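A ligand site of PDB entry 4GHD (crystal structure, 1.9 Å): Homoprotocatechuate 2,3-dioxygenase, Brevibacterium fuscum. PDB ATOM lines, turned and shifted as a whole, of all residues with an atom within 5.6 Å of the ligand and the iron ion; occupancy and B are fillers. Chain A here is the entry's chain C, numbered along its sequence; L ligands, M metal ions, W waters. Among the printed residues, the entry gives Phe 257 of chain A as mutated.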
ATOM      1  N   HIS A 155      35.175  19.688  -6.886  1.00  0.00           N
ATOM      2  CA  HIS A 155      35.520  18.421  -7.514  1.00  0.00           C
ATOM      3  C   HIS A 155      34.831  18.163  -8.810  1.00  0.00           C
ATOM      4  O   HIS A 155      33.936  18.919  -9.197  1.00  0.00           O
ATOM      5  CB  HIS A 155      35.246  17.261  -6.561  1.00  0.00           C
ATOM      6  CG  HIS A 155      33.808  17.079  -6.206  1.00  0.00           C
ATOM      7  ND1 HIS A 155      33.226  17.623  -5.084  1.00  0.00           N
ATOM      8  CD2 HIS A 155      32.809  16.393  -6.864  1.00  0.00           C
ATOM      9  CE1 HIS A 155      31.918  17.280  -5.051  1.00  0.00           C
ATOM     10  NE2 HIS A 155      31.655  16.547  -6.130  1.00  0.00           N
ATOM     11  N   ASN A 157      33.158  14.623 -11.052  1.00  0.00           N
ATOM     12  CA  ASN A 157      32.651  13.240 -10.930  1.00  0.00           C
ATOM     13  C   ASN A 157      32.474  12.688 -12.348  1.00  0.00           C
ATOM     14  O   ASN A 157      31.785  13.290 -13.186  1.00  0.00           O
ATOM     15  CB  ASN A 157      31.386  13.172 -10.091  1.00  0.00           C
ATOM     16  CG  ASN A 157      30.913  11.733  -9.822  1.00  0.00           C
ATOM     17  OD1 ASN A 157      30.685  10.959 -10.760  1.00  0.00           O
ATOM     18  ND2 ASN A 157      30.730  11.393  -8.530  1.00  0.00           N
ATOM     19  N   TRP A 192      35.482   7.659  -4.340  1.00  0.00           N
ATOM     20  CA  TRP A 192      35.800   9.087  -4.227  1.00  0.00           C
ATOM     21  C   TRP A 192      37.245   9.192  -3.882  1.00  0.00           C
ATOM     22  O   TRP A 192      37.712   8.433  -3.070  1.00  0.00           O
ATOM     23  CB  TRP A 192      34.970   9.701  -3.095  1.00  0.00           C
ATOM     24  CG  TRP A 192      33.537   9.979  -3.469  1.00  0.00           C
ATOM     25  CD1 TRP A 192      32.989  11.204  -3.814  1.00  0.00           C
ATOM     26  CD2 TRP A 192      32.418   9.027  -3.581  1.00  0.00           C
ATOM     27  NE1 TRP A 192      31.650  11.069  -4.093  1.00  0.00           N
ATOM     28  CE2 TRP A 192      31.254   9.803  -3.986  1.00  0.00           C
ATOM     29  CE3 TRP A 192      32.275   7.668  -3.377  1.00  0.00           C
ATOM     30  CZ2 TRP A 192      29.994   9.226  -4.131  1.00  0.00           C
ATOM     31  CZ3 TRP A 192      31.016   7.090  -3.554  1.00  0.00           C
ATOM     32  CH2 TRP A 192      29.908   7.862  -3.928  1.00  0.00           C
ATOM     33  N   HIS A 200      37.162  14.639  -1.934  1.00  0.00           N
ATOM     34  CA  HIS A 200      37.616  14.322  -3.282  1.00  0.00           C
ATOM     35  C   HIS A 200      37.969  15.479  -4.157  1.00  0.00           C
ATOM     36  O   HIS A 200      37.546  16.614  -3.930  1.00  0.00           O
ATOM     37  CB  HIS A 200      36.597  13.461  -3.997  1.00  0.00           C
ATOM     38  CG  HIS A 200      35.194  14.019  -4.031  1.00  0.00           C
ATOM     39  ND1 HIS A 200      34.583  14.566  -2.945  1.00  0.00           N
ATOM     40  CD2 HIS A 200      34.246  14.008  -5.055  1.00  0.00           C
ATOM     41  CE1 HIS A 200      33.312  14.870  -3.271  1.00  0.00           C
ATOM     42  NE2 HIS A 200      33.106  14.530  -4.552  1.00  0.00           N
ATOM     43  N   HIS A 214      29.235  15.326 -13.112  1.00  0.00           N
ATOM     44  CA  HIS A 214      29.050  16.718 -12.725  1.00  0.00           C
ATOM     45  C   HIS A 214      30.322  17.385 -12.394  1.00  0.00           C
ATOM     46  O   HIS A 214      31.368  16.734 -12.252  1.00  0.00           O
ATOM     47  CB  HIS A 214      28.094  16.838 -11.536  1.00  0.00           C
ATOM     48  CG  HIS A 214      28.532  16.106 -10.295  1.00  0.00           C
ATOM     49  ND1 HIS A 214      28.119  14.872  -9.990  1.00  0.00           N
ATOM     50  CD2 HIS A 214      29.336  16.509  -9.248  1.00  0.00           C
ATOM     51  CE1 HIS A 214      28.631  14.483  -8.820  1.00  0.00           C
ATOM     52  NE2 HIS A 214      29.407  15.458  -8.366  1.00  0.00           N
ATOM     53  N   ALA A 216      31.453  20.259  -9.359  1.00  0.00           N
ATOM     54  CA  ALA A 216      30.960  20.683  -8.052  1.00  0.00           C
ATOM     55  C   ALA A 216      31.651  21.922  -7.542  1.00  0.00           C
ATOM     56  O   ALA A 216      32.862  21.980  -7.528  1.00  0.00           O
ATOM     57  CB  ALA A 216      31.119  19.576  -7.043  1.00  0.00           C
ATOM     58  N   ARG A 243      17.881  17.125  -8.058  1.00  0.00           N
ATOM     59  CA  ARG A 243      17.938  16.313  -6.827  1.00  0.00           C
ATOM     60  C   ARG A 243      18.489  17.125  -5.658  1.00  0.00           C
ATOM     61  O   ARG A 243      19.497  17.811  -5.785  1.00  0.00           O
ATOM     62  CB  ARG A 243      18.831  15.112  -7.074  1.00  0.00           C
ATOM     63  CG  ARG A 243      19.172  14.278  -5.827  1.00  0.00           C
ATOM     64  CD  ARG A 243      19.990  13.043  -6.152  1.00  0.00           C
ATOM     65  NE  ARG A 243      20.406  12.504  -4.852  1.00  0.00           N
ATOM     66  CZ  ARG A 243      21.589  11.981  -4.590  1.00  0.00           C
ATOM     67  NH1 ARG A 243      22.497  11.746  -5.557  1.00  0.00           N
ATOM     68  NH2 ARG A 243      21.858  11.686  -3.353  1.00  0.00           N
ATOM     69  N   HIS A 248      24.539  14.376   2.321  1.00  0.00           N
ATOM     70  CA  HIS A 248      25.097  13.137   1.743  1.00  0.00           C
ATOM     71  C   HIS A 248      25.438  12.169   2.875  1.00  0.00           C
ATOM     72  O   HIS A 248      25.794  12.612   3.984  1.00  0.00           O
ATOM     73  CB  HIS A 248      26.412  13.436   1.031  1.00  0.00           C
ATOM     74  CG  HIS A 248      26.294  13.970  -0.368  1.00  0.00           C
ATOM     75  ND1 HIS A 248      25.553  13.357  -1.340  1.00  0.00           N
ATOM     76  CD2 HIS A 248      26.924  15.066  -0.965  1.00  0.00           C
ATOM     77  CE1 HIS A 248      25.693  14.034  -2.493  1.00  0.00           C
ATOM     78  NE2 HIS A 248      26.566  15.083  -2.260  1.00  0.00           N
ATOM     79  N   GLY A 249      25.375  10.861   2.637  1.00  0.00           N
ATOM     80  CA  GLY A 249      26.032   9.884   3.509  1.00  0.00           C
ATOM     81  C   GLY A 249      27.532   9.918   3.244  1.00  0.00           C
ATOM     82  O   GLY A 249      28.306  10.481   4.031  1.00  0.00           O
ATOM     83  N   VAL A 250      27.934   9.354   2.089  1.00  0.00           N
ATOM     84  CA  VAL A 250      29.260   9.561   1.562  1.00  0.00           C
ATOM     85  C   VAL A 250      29.632  11.035   1.539  1.00  0.00           C
ATOM     86  O   VAL A 250      28.955  11.849   0.895  1.00  0.00           O
ATOM     87  CB  VAL A 250      29.400   9.086   0.091  1.00  0.00           C
ATOM     88  CG1 VAL A 250      30.801   9.436  -0.490  1.00  0.00           C
ATOM     89  CG2 VAL A 250      29.098   7.579   0.000  1.00  0.00           C
ATOM     90  N   SER A 251      30.713  11.354   2.222  1.00  0.00           N
ATOM     91  CA  SER A 251      31.317  12.713   2.306  1.00  0.00           C
ATOM     92  C   SER A 251      30.733  13.579   3.451  1.00  0.00           C
ATOM     93  O   SER A 251      31.376  14.508   3.898  1.00  0.00           O
ATOM     94  CB  SER A 251      31.200  13.519   0.991  1.00  0.00           C
ATOM     95  OG  SER A 251      29.918  14.137   0.832  1.00  0.00           O
ATOM     96  N   TYR A 255      24.304  19.144   0.072  1.00  0.00           N
ATOM     97  CA  TYR A 255      24.413  19.117  -1.405  1.00  0.00           C
ATOM     98  C   TYR A 255      23.119  19.527  -2.120  1.00  0.00           C
ATOM     99  O   TYR A 255      22.042  19.430  -1.563  1.00  0.00           O
ATOM    100  CB  TYR A 255      24.813  17.723  -1.906  1.00  0.00           C
ATOM    101  CG  TYR A 255      23.707  16.693  -1.830  1.00  0.00           C
ATOM    102  CD1 TYR A 255      23.508  15.931  -0.663  1.00  0.00           C
ATOM    103  CD2 TYR A 255      22.860  16.461  -2.912  1.00  0.00           C
ATOM    104  CE1 TYR A 255      22.469  14.992  -0.599  1.00  0.00           C
ATOM    105  CE2 TYR A 255      21.836  15.519  -2.842  1.00  0.00           C
ATOM    106  CZ  TYR A 255      21.642  14.799  -1.698  1.00  0.00           C
ATOM    107  OH  TYR A 255      20.608  13.883  -1.609  1.00  0.00           O
ATOM    108  N   PHE A 257      21.917  19.141  -6.510  1.00  0.00           N
ATOM    109  CA  PHE A 257      22.200  18.974  -7.948  1.00  0.00           C
ATOM    110  C   PHE A 257      21.240  19.751  -8.850  1.00  0.00           C
ATOM    111  O   PHE A 257      20.003  19.600  -8.756  1.00  0.00           O
ATOM    112  CB  PHE A 257      22.170  17.524  -8.318  1.00  0.00           C
ATOM    113  CG  PHE A 257      23.218  16.695  -7.653  1.00  0.00           C
ATOM    114  CD1 PHE A 257      24.515  16.647  -8.159  1.00  0.00           C
ATOM    115  CD2 PHE A 257      22.916  15.977  -6.509  1.00  0.00           C
ATOM    116  CE1 PHE A 257      25.488  15.889  -7.526  1.00  0.00           C
ATOM    117  CE2 PHE A 257      23.861  15.190  -5.898  1.00  0.00           C
ATOM    118  CZ  PHE A 257      25.133  15.154  -6.387  1.00  0.00           C
ATOM    119  N   GLU A 267      26.908  20.290  -9.140  1.00  0.00           N
ATOM    120  CA  GLU A 267      26.622  20.080  -7.736  1.00  0.00           C
ATOM    121  C   GLU A 267      27.059  21.302  -6.942  1.00  0.00           C
ATOM    122  O   GLU A 267      28.126  21.894  -7.227  1.00  0.00           O
ATOM    123  CB  GLU A 267      27.307  18.833  -7.172  1.00  0.00           C
ATOM    124  CG  GLU A 267      26.940  18.533  -5.721  1.00  0.00           C
ATOM    125  CD  GLU A 267      27.680  17.330  -5.178  1.00  0.00           C
ATOM    126  OE1 GLU A 267      28.663  16.943  -5.807  1.00  0.00           O
ATOM    127  OE2 GLU A 267      27.250  16.775  -4.171  1.00  0.00           O
ATOM    128  N   TYR A 269      27.814  22.190  -2.916  1.00  0.00           N
ATOM    129  CA  TYR A 269      28.370  21.251  -1.943  1.00  0.00           C
ATOM    130  C   TYR A 269      28.982  22.041  -0.792  1.00  0.00           C
ATOM    131  O   TYR A 269      29.615  23.083  -1.037  1.00  0.00           O
ATOM    132  CB  TYR A 269      29.473  20.456  -2.679  1.00  0.00           C
ATOM    133  CG  TYR A 269      30.265  19.388  -1.979  1.00  0.00           C
ATOM    134  CD1 TYR A 269      29.891  18.038  -2.062  1.00  0.00           C
ATOM    135  CD2 TYR A 269      31.468  19.689  -1.333  1.00  0.00           C
ATOM    136  CE1 TYR A 269      30.651  17.055  -1.472  1.00  0.00           C
ATOM    137  CE2 TYR A 269      32.232  18.669  -0.742  1.00  0.00           C
ATOM    138  CZ  TYR A 269      31.822  17.361  -0.841  1.00  0.00           C
ATOM    139  OH  TYR A 269      32.586  16.343  -0.291  1.00  0.00           O
ATOM    140  N   ARG A 292      23.182   5.959   2.257  1.00  0.00           N
ATOM    141  CA  ARG A 292      24.576   6.149   1.714  1.00  0.00           C
ATOM    142  C   ARG A 292      24.705   7.352   0.788  1.00  0.00           C
ATOM    143  O   ARG A 292      25.760   7.969   0.730  1.00  0.00           O
ATOM    144  CB  ARG A 292      25.016   4.896   0.946  1.00  0.00           C
ATOM    145  CG  ARG A 292      24.469   4.798  -0.476  1.00  0.00           C
ATOM    146  CD  ARG A 292      24.411   3.399  -1.069  1.00  0.00           C
ATOM    147  NE  ARG A 292      23.776   3.489  -2.389  1.00  0.00           N
ATOM    148  CZ  ARG A 292      22.462   3.537  -2.620  1.00  0.00           C
ATOM    149  NH1 ARG A 292      21.574   3.476  -1.631  1.00  0.00           N
ATOM    150  NH2 ARG A 292      22.025   3.644  -3.858  1.00  0.00           N
ATOM    151  N   ARG A 293      23.649   7.675   0.049  1.00  0.00           N
ATOM    152  CA  ARG A 293      23.703   8.781  -0.906  1.00  0.00           C
ATOM    153  C   ARG A 293      22.986   9.957  -0.239  1.00  0.00           C
ATOM    154  O   ARG A 293      23.622  10.912   0.059  1.00  0.00           O
ATOM    155  CB  ARG A 293      23.180   8.426  -2.287  1.00  0.00           C
ATOM    156  CG  ARG A 293      24.161   7.527  -3.034  1.00  0.00           C
ATOM    157  CD  ARG A 293      23.906   7.443  -4.508  1.00  0.00           C
ATOM    158  NE  ARG A 293      24.891   6.676  -5.225  1.00  0.00           N
ATOM    159  CZ  ARG A 293      26.043   7.157  -5.708  1.00  0.00           C
ATOM    160  NH1 ARG A 293      26.384   8.407  -5.547  1.00  0.00           N
ATOM    161  NH2 ARG A 293      26.884   6.356  -6.343  1.00  0.00           N
ATOM    162  N   ASP A 294      21.718   9.824   0.054  1.00  0.00           N
ATOM    163  CA  ASP A 294      21.065  10.818   0.865  1.00  0.00           C
ATOM    164  C   ASP A 294      20.893  10.266   2.262  1.00  0.00           C
ATOM    165  O   ASP A 294      20.232   9.256   2.468  1.00  0.00           O
ATOM    166  CB  ASP A 294      19.716  11.185   0.276  1.00  0.00           C
ATOM    167  CG  ASP A 294      19.097  12.400   0.954  1.00  0.00           C
ATOM    168  OD1 ASP A 294      19.483  13.559   0.605  1.00  0.00           O
ATOM    169  OD2 ASP A 294      18.224  12.201   1.835  1.00  0.00           O
ATOM    170  N   VAL A 300      16.858   8.597  -4.716  1.00  0.00           N
ATOM    171  CA  VAL A 300      17.706   9.131  -5.796  1.00  0.00           C
ATOM    172  C   VAL A 300      16.967   8.932  -7.142  1.00  0.00           C
ATOM    173  O   VAL A 300      16.677   7.825  -7.551  1.00  0.00           O
ATOM    174  CB  VAL A 300      19.063   8.429  -5.818  1.00  0.00           C
ATOM    175  CG1 VAL A 300      19.889   8.915  -6.999  1.00  0.00           C
ATOM    176  CG2 VAL A 300      19.810   8.635  -4.472  1.00  0.00           C
ATOM    177  N   TRP A 304      19.609  10.736 -12.182  1.00  0.00           N
ATOM    178  CA  TRP A 304      20.935  10.926 -11.544  1.00  0.00           C
ATOM    179  C   TRP A 304      21.883   9.801 -11.930  1.00  0.00           C
ATOM    180  O   TRP A 304      23.059   9.994 -12.160  1.00  0.00           O
ATOM    181  CB  TRP A 304      20.760  11.061 -10.030  1.00  0.00           C
ATOM    182  CG  TRP A 304      21.963  11.711  -9.387  1.00  0.00           C
ATOM    183  CD1 TRP A 304      22.182  13.054  -9.172  1.00  0.00           C
ATOM    184  CD2 TRP A 304      23.159  11.036  -8.924  1.00  0.00           C
ATOM    185  NE1 TRP A 304      23.424  13.251  -8.631  1.00  0.00           N
ATOM    186  CE2 TRP A 304      24.069  12.069  -8.461  1.00  0.00           C
ATOM    187  CE3 TRP A 304      23.583   9.730  -8.929  1.00  0.00           C
ATOM    188  CZ2 TRP A 304      25.323  11.798  -7.978  1.00  0.00           C
ATOM    189  CZ3 TRP A 304      24.846   9.447  -8.429  1.00  0.00           C
ATOM    190  CH2 TRP A 304      25.711  10.457  -7.974  1.00  0.00           C
HETATM  191  C1  LIG L   1      27.631  11.627  -3.163  1.00  0.00           C
HETATM  192  C2  LIG L   1      27.546  12.275  -4.459  1.00  0.00           C
HETATM  193  C3  LIG L   1      28.336  13.427  -4.740  1.00  0.00           C
HETATM  194  C4  LIG L   1      29.230  13.924  -3.730  1.00  0.00           C
HETATM  195  C5  LIG L   1      29.334  13.241  -2.477  1.00  0.00           C
HETATM  196  C6  LIG L   1      28.501  12.123  -2.170  1.00  0.00           C
HETATM  197  C7  LIG L   1      26.692  10.449  -2.902  1.00  0.00           C
HETATM  198  C8  LIG L   1      25.246  10.910  -3.347  1.00  0.00           C
HETATM  199  O1  LIG L   1      24.524  11.543  -2.585  1.00  0.00           O
HETATM  200  O2  LIG L   1      24.918  10.677  -4.434  1.00  0.00           O
HETATM  201  O3  LIG L   1      28.230  14.005  -5.943  1.00  0.00           O
HETATM  202  O4  LIG L   1      30.041  15.021  -3.964  1.00  0.00           O
HETATM  203 FE    FE M   1      29.845  15.246  -6.161  1.00  0.00          FE
HETATM  204  O   HOH W   1      31.151  13.282  -6.369  1.00  0.00           O
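The guanidinium group of Arg 243 is in salt-bridge range of an oxygen (O1) of the ligand, 2.8 Å away.
The guanidinium group of Arg 293 lies within salt-bridge range of an oxygen (O2) of the ligand (2.9 Å).
NE2 of His 200 sits close to O4 of the ligand (3.2 Å).
A ring nitrogen (ND1) of His 248 sits at hydrogen-bond distance from an oxygen (O1) of the ligand, 2.4 Å away.
An oxygen (O1) of the ligand sits close to the backbone carbonyl oxygen (O) of Arg 293.
N of Ala 216 is in hydrogen-bond range of O of His 155, 2.8 Å away.
OE2 of Glu 267 sits at hydrogen-bond distance from NE2 of His 248 (2.6 Å).
OH of Tyr 255 sits at hydrogen-bond distance from NH2 of Arg 243, at 3.1 Å.
A ring nitrogen (ND1) of His 248 lies close to the backbone carbonyl oxygen (O) of Arg 293 (3.4 Å).
A ring nitrogen (ND1) of His 155 sits close to a ring nitrogen (NE2) of His 200 (3.1 Å).
O of Arg 293 lies within hydrogen-bond range of N of Gly 249, at 3.1 Å.
The backbone carbonyl oxygen (O) of His 214 is in hydrogen-bond range of the backbone NH (N) of Asn 157 (3.0 Å).
N of Phe 257 sits at hydrogen-bond distance from O of Arg 243, at 2.9 Å.
Trp 192 touches the ligand.
Val 250 touches the ligand.
Ser 251 touches the ligand (OG to C5, 3.5 Å).
Phe 257 touches the ligand.
Tyr 269 touches the ligand (CE1 to O4, 3.3 Å).
Trp 304 touches the ligand (CH2 to O2, 3.6 Å).
Hydrophobic or aromatic side chains that line the ligand: His 155, Trp 192, His 200, His 214, His 248, Val 250, Phe 257, Tyr 269 and Trp 304.
Residues that only touch the iron ion: His 200 (3.7 Å).
Of the 20 residues printed, 4 come within 4 Å of the iron ion.
The nearest printed residue that does not touch the iron ion is Ala 216 (4.6 Å).
The iron ion is bound by an oxygen (O3) of the ligand.
The iron ion is bound by the side-chain carboxylate (OE1) of Glu 267 (2.1 Å).
O4 of the ligand is bound to the iron ion, 2.2 Å away.
A ring nitrogen (NE2) of His 155 binds the iron ion, at 2.2 Å.
NE2 of His 214 binds the iron ion, at 2.3 Å.
Water W1 is bound to the iron ion (2.4 Å).
Water W1 lies within hydrogen-bond range of ND2 of Asn 157 (2.9 Å), NE2 of His 200 (2.9 Å) and NE1 of Trp 192 (3.2 Å).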
